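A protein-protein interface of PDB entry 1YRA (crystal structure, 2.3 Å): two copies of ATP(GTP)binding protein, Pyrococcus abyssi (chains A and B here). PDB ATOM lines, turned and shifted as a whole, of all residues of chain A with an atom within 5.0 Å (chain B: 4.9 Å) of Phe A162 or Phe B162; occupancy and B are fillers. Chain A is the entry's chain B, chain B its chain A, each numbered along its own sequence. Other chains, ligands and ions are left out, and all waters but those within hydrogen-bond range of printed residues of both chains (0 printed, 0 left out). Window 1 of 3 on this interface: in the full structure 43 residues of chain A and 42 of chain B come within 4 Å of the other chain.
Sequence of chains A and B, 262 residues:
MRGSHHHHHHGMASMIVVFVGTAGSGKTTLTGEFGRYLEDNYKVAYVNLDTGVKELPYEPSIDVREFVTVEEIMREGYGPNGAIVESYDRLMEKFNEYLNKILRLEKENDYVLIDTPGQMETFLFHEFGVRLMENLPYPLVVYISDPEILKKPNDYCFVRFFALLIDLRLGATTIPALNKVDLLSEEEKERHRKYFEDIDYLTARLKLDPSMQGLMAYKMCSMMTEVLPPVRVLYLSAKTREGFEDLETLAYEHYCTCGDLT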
ATOM      1  N   MET A 120       0.734  29.718  -9.584  1.00  0.00           N
ATOM      2  CA  MET A 120       0.826  30.514  -8.376  1.00  0.00           C
ATOM      3  C   MET A 120       1.738  29.908  -7.309  1.00  0.00           C
ATOM      4  O   MET A 120       2.448  30.625  -6.590  1.00  0.00           O
ATOM      5  CB  MET A 120      -0.582  30.605  -7.823  1.00  0.00           C
ATOM      6  CG  MET A 120      -0.726  31.432  -6.621  1.00  0.00           C
ATOM      7  SD  MET A 120      -2.451  31.834  -6.478  1.00  0.00           S
ATOM      8  CE  MET A 120      -3.206  30.222  -6.400  1.00  0.00           C
ATOM      9  N   LEU A 124       4.625  31.243  -4.830  1.00  0.00           N
ATOM     10  CA  LEU A 124       4.384  31.299  -3.396  1.00  0.00           C
ATOM     11  C   LEU A 124       5.311  30.383  -2.583  1.00  0.00           C
ATOM     12  O   LEU A 124       5.578  30.650  -1.401  1.00  0.00           O
ATOM     13  CB  LEU A 124       2.911  30.990  -3.100  1.00  0.00           C
ATOM     14  CG  LEU A 124       1.901  32.073  -3.531  1.00  0.00           C
ATOM     15  CD1 LEU A 124       0.461  31.612  -3.315  1.00  0.00           C
ATOM     16  CD2 LEU A 124       2.124  33.389  -2.791  1.00  0.00           C
ATOM     17  N   PHE A 125       5.812  29.313  -3.201  1.00  0.00           N
ATOM     18  CA  PHE A 125       6.566  28.307  -2.440  1.00  0.00           C
ATOM     19  C   PHE A 125       8.037  28.233  -2.807  1.00  0.00           C
ATOM     20  O   PHE A 125       8.825  27.639  -2.080  1.00  0.00           O
ATOM     21  CB  PHE A 125       5.921  26.927  -2.562  1.00  0.00           C
ATOM     22  CG  PHE A 125       4.542  26.829  -1.934  1.00  0.00           C
ATOM     23  CD1 PHE A 125       4.374  26.251  -0.675  1.00  0.00           C
ATOM     24  CD2 PHE A 125       3.430  27.308  -2.603  1.00  0.00           C
ATOM     25  CE1 PHE A 125       3.118  26.149  -0.082  1.00  0.00           C
ATOM     26  CE2 PHE A 125       2.167  27.229  -2.028  1.00  0.00           C
ATOM     27  CZ  PHE A 125       2.004  26.641  -0.759  1.00  0.00           C
ATOM     28  N   TYR A 143      -4.477  39.736  -6.544  1.00  0.00           N
ATOM     29  CA  TYR A 143      -4.775  38.315  -6.604  1.00  0.00           C
ATOM     30  C   TYR A 143      -6.096  38.045  -7.301  1.00  0.00           C
ATOM     31  O   TYR A 143      -7.141  38.227  -6.711  1.00  0.00           O
ATOM     32  CB  TYR A 143      -4.712  37.664  -5.217  1.00  0.00           C
ATOM     33  CG  TYR A 143      -5.344  36.299  -5.197  1.00  0.00           C
ATOM     34  CD1 TYR A 143      -4.894  35.283  -6.040  1.00  0.00           C
ATOM     35  CD2 TYR A 143      -6.402  36.018  -4.337  1.00  0.00           C
ATOM     36  CE1 TYR A 143      -5.487  34.028  -6.018  1.00  0.00           C
ATOM     37  CE2 TYR A 143      -6.989  34.776  -4.309  1.00  0.00           C
ATOM     38  CZ  TYR A 143      -6.535  33.788  -5.142  1.00  0.00           C
ATOM     39  OH  TYR A 143      -7.161  32.557  -5.112  1.00  0.00           O
ATOM     40  N   CYS A 157     -15.228  32.668   1.415  1.00  0.00           N
ATOM     41  CA  CYS A 157     -14.302  32.653   2.550  1.00  0.00           C
ATOM     42  C   CYS A 157     -12.937  32.146   2.090  1.00  0.00           C
ATOM     43  O   CYS A 157     -11.921  32.795   2.297  1.00  0.00           O
ATOM     44  CB  CYS A 157     -14.834  31.745   3.681  1.00  0.00           C
ATOM     45  SG  CYS A 157     -13.805  31.738   5.200  1.00  0.00           S
ATOM     46  N   PHE A 158     -12.947  30.976   1.457  1.00  0.00           N
ATOM     47  CA  PHE A 158     -11.758  30.331   0.944  1.00  0.00           C
ATOM     48  C   PHE A 158     -10.874  31.278   0.130  1.00  0.00           C
ATOM     49  O   PHE A 158      -9.667  31.361   0.340  1.00  0.00           O
ATOM     50  CB  PHE A 158     -12.176  29.133   0.094  1.00  0.00           C
ATOM     51  CG  PHE A 158     -11.074  28.564  -0.757  1.00  0.00           C
ATOM     52  CD1 PHE A 158      -9.928  28.029  -0.176  1.00  0.00           C
ATOM     53  CD2 PHE A 158     -11.194  28.534  -2.140  1.00  0.00           C
ATOM     54  CE1 PHE A 158      -8.903  27.500  -0.963  1.00  0.00           C
ATOM     55  CE2 PHE A 158     -10.177  28.004  -2.929  1.00  0.00           C
ATOM     56  CZ  PHE A 158      -9.032  27.482  -2.331  1.00  0.00           C
ATOM     57  N   VAL A 159     -11.489  32.005  -0.787  1.00  0.00           N
ATOM     58  CA  VAL A 159     -10.762  32.857  -1.697  1.00  0.00           C
ATOM     59  C   VAL A 159     -10.262  34.121  -1.019  1.00  0.00           C
ATOM     60  O   VAL A 159      -9.207  34.640  -1.383  1.00  0.00           O
ATOM     61  CB  VAL A 159     -11.627  33.179  -2.928  1.00  0.00           C
ATOM     62  CG1 VAL A 159     -11.156  34.428  -3.612  1.00  0.00           C
ATOM     63  CG2 VAL A 159     -11.624  31.979  -3.881  1.00  0.00           C
ATOM     64  N   ARG A 160     -11.001  34.624  -0.031  1.00  0.00           N
ATOM     65  CA  ARG A 160     -10.547  35.809   0.704  1.00  0.00           C
ATOM     66  C   ARG A 160      -9.493  35.454   1.758  1.00  0.00           C
ATOM     67  O   ARG A 160      -8.560  36.207   2.015  1.00  0.00           O
ATOM     68  CB  ARG A 160     -11.745  36.540   1.328  1.00  0.00           C
ATOM     69  CG  ARG A 160     -12.221  37.801   0.546  1.00  0.00           C
ATOM     70  CD  ARG A 160     -11.269  38.998   0.848  1.00  0.00           C
ATOM     71  NE  ARG A 160     -11.898  40.325   0.816  1.00  0.00           N
ATOM     72  CZ  ARG A 160     -13.163  40.584   1.146  1.00  0.00           C
ATOM     73  NH1 ARG A 160     -13.959  39.617   1.577  1.00  0.00           N
ATOM     74  NH2 ARG A 160     -13.636  41.823   1.061  1.00  0.00           N
ATOM     75  N   PHE A 161      -9.638  34.300   2.387  1.00  0.00           N
ATOM     76  CA  PHE A 161      -8.584  33.852   3.276  1.00  0.00           C
ATOM     77  C   PHE A 161      -7.286  33.612   2.488  1.00  0.00           C
ATOM     78  O   PHE A 161      -6.216  34.083   2.875  1.00  0.00           O
ATOM     79  CB  PHE A 161      -9.012  32.622   4.061  1.00  0.00           C
ATOM     80  CG  PHE A 161      -8.306  32.479   5.374  1.00  0.00           C
ATOM     81  CD1 PHE A 161      -7.130  31.732   5.475  1.00  0.00           C
ATOM     82  CD2 PHE A 161      -8.812  33.091   6.517  1.00  0.00           C
ATOM     83  CE1 PHE A 161      -6.465  31.603   6.685  1.00  0.00           C
ATOM     84  CE2 PHE A 161      -8.155  32.959   7.750  1.00  0.00           C
ATOM     85  CZ  PHE A 161      -6.972  32.216   7.828  1.00  0.00           C
ATOM     86  N   PHE A 162      -7.390  32.954   1.345  1.00  0.00           N
ATOM     87  CA  PHE A 162      -6.232  32.755   0.487  1.00  0.00           C
ATOM     88  C   PHE A 162      -5.441  34.040   0.221  1.00  0.00           C
ATOM     89  O   PHE A 162      -4.204  34.044   0.296  1.00  0.00           O
ATOM     90  CB  PHE A 162      -6.633  32.084  -0.843  1.00  0.00           C
ATOM     91  CG  PHE A 162      -5.496  31.378  -1.503  1.00  0.00           C
ATOM     92  CD1 PHE A 162      -5.151  30.098  -1.130  1.00  0.00           C
ATOM     93  CD2 PHE A 162      -4.735  32.006  -2.454  1.00  0.00           C
ATOM     94  CE1 PHE A 162      -4.066  29.449  -1.719  1.00  0.00           C
ATOM     95  CE2 PHE A 162      -3.642  31.361  -3.040  1.00  0.00           C
ATOM     96  CZ  PHE A 162      -3.318  30.089  -2.677  1.00  0.00           C
ATOM     97  N   ALA A 163      -6.158  35.106  -0.115  1.00  0.00           N
ATOM     98  CA  ALA A 163      -5.572  36.423  -0.401  1.00  0.00           C
ATOM     99  C   ALA A 163      -4.792  36.877   0.797  1.00  0.00           C
ATOM    100  O   ALA A 163      -3.683  37.407   0.684  1.00  0.00           O
ATOM    101  CB  ALA A 163      -6.686  37.458  -0.733  1.00  0.00           C
ATOM    102  N   LEU A 164      -5.392  36.651   1.965  1.00  0.00           N
ATOM    103  CA  LEU A 164      -4.747  36.943   3.228  1.00  0.00           C
ATOM    104  C   LEU A 164      -3.448  36.147   3.303  1.00  0.00           C
ATOM    105  O   LEU A 164      -2.405  36.679   3.706  1.00  0.00           O
ATOM    106  CB  LEU A 164      -5.683  36.565   4.389  1.00  0.00           C
ATOM    107  CG  LEU A 164      -5.248  36.972   5.786  1.00  0.00           C
ATOM    108  CD1 LEU A 164      -4.736  38.408   5.761  1.00  0.00           C
ATOM    109  CD2 LEU A 164      -6.403  36.825   6.783  1.00  0.00           C
ATOM    110  N   LEU A 165      -3.511  34.873   2.921  1.00  0.00           N
ATOM    111  CA  LEU A 165      -2.313  34.027   2.949  1.00  0.00           C
ATOM    112  C   LEU A 165      -1.236  34.527   1.996  1.00  0.00           C
ATOM    113  O   LEU A 165      -0.060  34.410   2.277  1.00  0.00           O
ATOM    114  CB  LEU A 165      -2.637  32.547   2.645  1.00  0.00           C
ATOM    115  CG  LEU A 165      -2.870  31.617   3.850  1.00  0.00           C
ATOM    116  CD1 LEU A 165      -3.708  32.315   4.873  1.00  0.00           C
ATOM    117  CD2 LEU A 165      -3.519  30.300   3.464  1.00  0.00           C
ATOM    118  N   ILE A 166      -1.639  35.064   0.854  1.00  0.00           N
ATOM    119  CA  ILE A 166      -0.673  35.622  -0.066  1.00  0.00           C
ATOM    120  C   ILE A 166       0.022  36.819   0.588  1.00  0.00           C
ATOM    121  O   ILE A 166       1.246  36.930   0.587  1.00  0.00           O
ATOM    122  CB  ILE A 166      -1.350  36.027  -1.406  1.00  0.00           C
ATOM    123  CG1 ILE A 166      -1.968  34.783  -2.065  1.00  0.00           C
ATOM    124  CG2 ILE A 166      -0.343  36.724  -2.318  1.00  0.00           C
ATOM    125  CD1 ILE A 166      -2.766  35.043  -3.291  1.00  0.00           C
ATOM    126  N   MET B 120      -0.521  21.448  -6.609  1.00  0.00           N
ATOM    127  CA  MET B 120      -1.564  21.596  -5.603  1.00  0.00           C
ATOM    128  C   MET B 120      -2.735  22.516  -6.043  1.00  0.00           C
ATOM    129  O   MET B 120      -3.887  22.279  -5.673  1.00  0.00           O
ATOM    130  CB  MET B 120      -0.923  22.120  -4.330  1.00  0.00           C
ATOM    131  CG  MET B 120      -1.811  22.186  -3.136  1.00  0.00           C
ATOM    132  SD  MET B 120      -0.765  22.477  -1.697  1.00  0.00           S
ATOM    133  CE  MET B 120       0.173  23.902  -2.237  1.00  0.00           C
ATOM    134  N   LEU B 124      -6.868  22.187  -5.682  1.00  0.00           N
ATOM    135  CA  LEU B 124      -7.555  23.083  -4.756  1.00  0.00           C
ATOM    136  C   LEU B 124      -8.475  24.096  -5.442  1.00  0.00           C
ATOM    137  O   LEU B 124      -9.426  24.561  -4.841  1.00  0.00           O
ATOM    138  CB  LEU B 124      -6.532  23.832  -3.893  1.00  0.00           C
ATOM    139  CG  LEU B 124      -5.703  22.982  -2.914  1.00  0.00           C
ATOM    140  CD1 LEU B 124      -4.745  23.891  -2.170  1.00  0.00           C
ATOM    141  CD2 LEU B 124      -6.601  22.239  -1.937  1.00  0.00           C
ATOM    142  N   PHE B 125      -8.166  24.462  -6.682  1.00  0.00           N
ATOM    143  CA  PHE B 125      -8.938  25.485  -7.384  1.00  0.00           C
ATOM    144  C   PHE B 125      -9.667  24.938  -8.614  1.00  0.00           C
ATOM    145  O   PHE B 125     -10.318  25.683  -9.335  1.00  0.00           O
ATOM    146  CB  PHE B 125      -8.034  26.640  -7.805  1.00  0.00           C
ATOM    147  CG  PHE B 125      -7.410  27.376  -6.651  1.00  0.00           C
ATOM    148  CD1 PHE B 125      -8.054  28.466  -6.075  1.00  0.00           C
ATOM    149  CD2 PHE B 125      -6.183  26.989  -6.151  1.00  0.00           C
ATOM    150  CE1 PHE B 125      -7.473  29.157  -5.008  1.00  0.00           C
ATOM    151  CE2 PHE B 125      -5.600  27.660  -5.081  1.00  0.00           C
ATOM    152  CZ  PHE B 125      -6.255  28.745  -4.506  1.00  0.00           C
ATOM    153  N   TYR B 143      -1.156  16.864   4.170  1.00  0.00           N
ATOM    154  CA  TYR B 143      -0.552  18.017   3.502  1.00  0.00           C
ATOM    155  C   TYR B 143       0.945  18.128   3.827  1.00  0.00           C
ATOM    156  O   TYR B 143       1.305  18.440   4.969  1.00  0.00           O
ATOM    157  CB  TYR B 143      -1.268  19.305   3.919  1.00  0.00           C
ATOM    158  CG  TYR B 143      -0.503  20.561   3.572  1.00  0.00           C
ATOM    159  CD1 TYR B 143      -0.117  20.814   2.266  1.00  0.00           C
ATOM    160  CD2 TYR B 143      -0.183  21.502   4.543  1.00  0.00           C
ATOM    161  CE1 TYR B 143       0.555  21.939   1.936  1.00  0.00           C
ATOM    162  CE2 TYR B 143       0.490  22.647   4.213  1.00  0.00           C
ATOM    163  CZ  TYR B 143       0.856  22.848   2.908  1.00  0.00           C
ATOM    164  OH  TYR B 143       1.530  23.983   2.545  1.00  0.00           O
ATOM    165  N   CYS B 157       3.564  29.750  10.575  1.00  0.00           N
ATOM    166  CA  CYS B 157       2.162  30.147  10.668  1.00  0.00           C
ATOM    167  C   CYS B 157       1.515  30.000   9.284  1.00  0.00           C
ATOM    168  O   CYS B 157       0.353  29.572   9.156  1.00  0.00           O
ATOM    169  CB  CYS B 157       2.095  31.591  11.189  1.00  0.00           C
ATOM    170  SG  CYS B 157       0.491  32.414  11.168  1.00  0.00           S
ATOM    171  N   PHE B 158       2.289  30.332   8.254  1.00  0.00           N
ATOM    172  CA  PHE B 158       1.869  30.128   6.864  1.00  0.00           C
ATOM    173  C   PHE B 158       1.428  28.681   6.594  1.00  0.00           C
ATOM    174  O   PHE B 158       0.274  28.431   6.243  1.00  0.00           O
ATOM    175  CB  PHE B 158       2.995  30.516   5.903  1.00  0.00           C
ATOM    176  CG  PHE B 158       2.707  30.169   4.467  1.00  0.00           C
ATOM    177  CD1 PHE B 158       1.658  30.773   3.790  1.00  0.00           C
ATOM    178  CD2 PHE B 158       3.495  29.246   3.787  1.00  0.00           C
ATOM    179  CE1 PHE B 158       1.402  30.461   2.466  1.00  0.00           C
ATOM    180  CE2 PHE B 158       3.237  28.931   2.470  1.00  0.00           C
ATOM    181  CZ  PHE B 158       2.188  29.535   1.813  1.00  0.00           C
ATOM    182  N   VAL B 159       2.351  27.739   6.786  1.00  0.00           N
ATOM    183  CA  VAL B 159       2.060  26.310   6.623  1.00  0.00           C
ATOM    184  C   VAL B 159       0.836  25.851   7.416  1.00  0.00           C
ATOM    185  O   VAL B 159       0.018  25.086   6.880  1.00  0.00           O
ATOM    186  CB  VAL B 159       3.215  25.454   7.070  1.00  0.00           C
ATOM    187  CG1 VAL B 159       2.776  23.983   7.184  1.00  0.00           C
ATOM    188  CG2 VAL B 159       4.381  25.606   6.117  1.00  0.00           C
ATOM    189  N   ARG B 160       0.718  26.294   8.678  1.00  0.00           N
ATOM    190  CA  ARG B 160      -0.389  25.890   9.528  1.00  0.00           C
ATOM    191  C   ARG B 160      -1.725  26.406   9.000  1.00  0.00           C
ATOM    192  O   ARG B 160      -2.710  25.680   8.985  1.00  0.00           O
ATOM    193  CB  ARG B 160      -0.188  26.399  10.954  1.00  0.00           C
ATOM    194  CG  ARG B 160       0.606  25.481  11.875  1.00  0.00           C
ATOM    195  CD  ARG B 160       0.204  25.691  13.333  1.00  0.00           C
ATOM    196  NE  ARG B 160       0.885  24.748  14.228  1.00  0.00           N
ATOM    197  CZ  ARG B 160       0.639  23.435  14.268  1.00  0.00           C
ATOM    198  NH1 ARG B 160      -0.275  22.897  13.471  1.00  0.00           N
ATOM    199  NH2 ARG B 160       1.296  22.660  15.123  1.00  0.00           N
ATOM    200  N   PHE B 161      -1.756  27.669   8.582  1.00  0.00           N
ATOM    201  CA  PHE B 161      -2.972  28.268   8.037  1.00  0.00           C
ATOM    202  C   PHE B 161      -3.316  27.737   6.657  1.00  0.00           C
ATOM    203  O   PHE B 161      -4.485  27.646   6.297  1.00  0.00           O
ATOM    204  CB  PHE B 161      -2.938  29.807   8.104  1.00  0.00           C
ATOM    205  CG  PHE B 161      -3.371  30.327   9.435  1.00  0.00           C
ATOM    206  CD1 PHE B 161      -4.721  30.440   9.736  1.00  0.00           C
ATOM    207  CD2 PHE B 161      -2.430  30.603  10.436  1.00  0.00           C
ATOM    208  CE1 PHE B 161      -5.140  30.885  10.994  1.00  0.00           C
ATOM    209  CE2 PHE B 161      -2.824  31.045  11.688  1.00  0.00           C
ATOM    210  CZ  PHE B 161      -4.182  31.188  11.977  1.00  0.00           C
ATOM    211  N   PHE B 162      -2.300  27.344   5.899  1.00  0.00           N
ATOM    212  CA  PHE B 162      -2.563  26.733   4.609  1.00  0.00           C
ATOM    213  C   PHE B 162      -3.245  25.364   4.758  1.00  0.00           C
ATOM    214  O   PHE B 162      -4.174  25.024   4.013  1.00  0.00           O
ATOM    215  CB  PHE B 162      -1.300  26.624   3.771  1.00  0.00           C
ATOM    216  CG  PHE B 162      -1.576  26.526   2.301  1.00  0.00           C
ATOM    217  CD1 PHE B 162      -1.578  27.656   1.510  1.00  0.00           C
ATOM    218  CD2 PHE B 162      -1.861  25.312   1.721  1.00  0.00           C
ATOM    219  CE1 PHE B 162      -1.847  27.565   0.171  1.00  0.00           C
ATOM    220  CE2 PHE B 162      -2.141  25.211   0.390  1.00  0.00           C
ATOM    221  CZ  PHE B 162      -2.134  26.332  -0.388  1.00  0.00           C
ATOM    222  N   ALA B 163      -2.801  24.592   5.732  1.00  0.00           N
ATOM    223  CA  ALA B 163      -3.457  23.320   6.018  1.00  0.00           C
ATOM    224  C   ALA B 163      -4.931  23.516   6.400  1.00  0.00           C
ATOM    225  O   ALA B 163      -5.831  22.794   5.918  1.00  0.00           O
ATOM    226  CB  ALA B 163      -2.683  22.552   7.109  1.00  0.00           C
ATOM    227  N   LEU B 164      -5.184  24.492   7.262  1.00  0.00           N
ATOM    228  CA  LEU B 164      -6.557  24.869   7.618  1.00  0.00           C
ATOM    229  C   LEU B 164      -7.361  25.231   6.361  1.00  0.00           C
ATOM    230  O   LEU B 164      -8.538  24.853   6.206  1.00  0.00           O
ATOM    231  CB  LEU B 164      -6.550  26.058   8.596  1.00  0.00           C
ATOM    232  CG  LEU B 164      -6.517  25.774  10.111  1.00  0.00           C
ATOM    233  CD1 LEU B 164      -5.448  24.764  10.483  1.00  0.00           C
ATOM    234  CD2 LEU B 164      -6.331  27.067  10.957  1.00  0.00           C
ATOM    235  N   LEU B 165      -6.713  25.962   5.463  1.00  0.00           N
ATOM    236  CA  LEU B 165      -7.362  26.416   4.251  1.00  0.00           C
ATOM    237  C   LEU B 165      -7.736  25.197   3.449  1.00  0.00           C
ATOM    238  O   LEU B 165      -8.842  25.120   2.909  1.00  0.00           O
ATOM    239  CB  LEU B 165      -6.439  27.309   3.434  1.00  0.00           C
ATOM    240  CG  LEU B 165      -7.179  28.143   2.388  1.00  0.00           C
ATOM    241  CD1 LEU B 165      -8.003  29.206   3.125  1.00  0.00           C
ATOM    242  CD2 LEU B 165      -6.221  28.789   1.390  1.00  0.00           C
ATOM    243  N   ILE B 166      -6.824  24.227   3.410  1.00  0.00           N
ATOM    244  CA  ILE B 166      -7.035  23.001   2.656  1.00  0.00           C
ATOM    245  C   ILE B 166      -8.186  22.218   3.275  1.00  0.00           C
ATOM    246  O   ILE B 166      -9.051  21.683   2.583  1.00  0.00           O
ATOM    247  CB  ILE B 166      -5.765  22.103   2.645  1.00  0.00           C
ATOM    248  CG1 ILE B 166      -4.690  22.703   1.731  1.00  0.00           C
ATOM    249  CG2 ILE B 166      -6.159  20.681   2.234  1.00  0.00           C
ATOM    250  CD1 ILE B 166      -3.344  22.000   1.775  1.00  0.00           C
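Of the printed residues of chain B, Phe A161 touches Phe B161 and Leu B165.
Phe A162 touches three residues of chain B.
Printed residues of chain A within 4 Å of Phe B161: Phe A161 (3.4 Å).
Printed residues of chain A within 4 Å of Phe B162: Phe A162 and Leu A165.
The nearest printed residue of chain B that does not touch Phe A162 is Leu B124 (5.6 Å).
The nearest residue of chain A that does not touch Phe B162 is Phe A125 (4.1 Å).
The nearest printed residue of chain B that does not touch Phe A125 is Phe B162 (4.1 Å).
Phe A125 touches Tyr B143, and with the chains exchanged Tyr A143 touches Phe B125.
Phe A158 touches Leu B124, but with the chains exchanged Leu A124 does not touch Phe B158 (4.8 Å).
Phe A161 touches Leu B165, but with the chains exchanged Leu A165 does not touch Phe B161 (4.0003 Å).
Phe A162 touches Leu B165, and with the chains exchanged Leu A165 touches Phe B162.
14 positions are printed for both chains.
Of the 15 pairs that touch across the chains among the printed residues, 11 have their exchanged pair printed and touching as well.
Among the printed residues, pairs that only touch across the chains: Phe A162 with Leu B165 (3.0 Å), Tyr A143 with Phe B125 (3.4 Å), Phe A161 with Phe B161 (3.4 Å), Phe A162 with Phe B162 (3.5 Å), Phe A158 with Phe B125 (3.5 Å), Phe A161 with Leu B165 (3.6 Å), Phe A125 with Met B120 (3.6 Å), Phe A162 with Phe B125 (3.6 Å), Leu A165 with Leu B165 (3.7 Å), Met A120 with Phe B125 (3.7 Å), Phe A125 with Tyr B143 (3.8 Å), Phe A158 with Leu B165 (3.8 Å), Phe A125 with Phe B158 (3.8 Å), Leu A165 with Phe B162 (3.8 Å) and Phe A158 with Leu B124 (3.9 Å).
Printed residues of chain A that touch a printed residue of chain B: Met A120, Phe A125, Tyr A143, Phe A158, Phe A161, Phe A162 and Leu A165.
Hydrophobic or aromatic side chains of chain A within 4 Å of the printed part of chain B: Met A120, Phe A125, Tyr A143, Phe A158, Phe A161, Phe A162 and Leu A165.
Of the 14 printed residues of chain B, 8 touch a printed residue of chain A.
Hydrophobic or aromatic side chains of chain B that line the printed part of chain A: Met B120, Phe B125, Tyr B143, Phe B158, Phe B161, Phe B162 and Leu B165.
Among the printed residues, 15 pairs touch across the chains.
Among the printed residues, no Asp or Glu carboxylate lies within 4 Å of a Lys or Arg side-chain nitrogen of the other chain.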
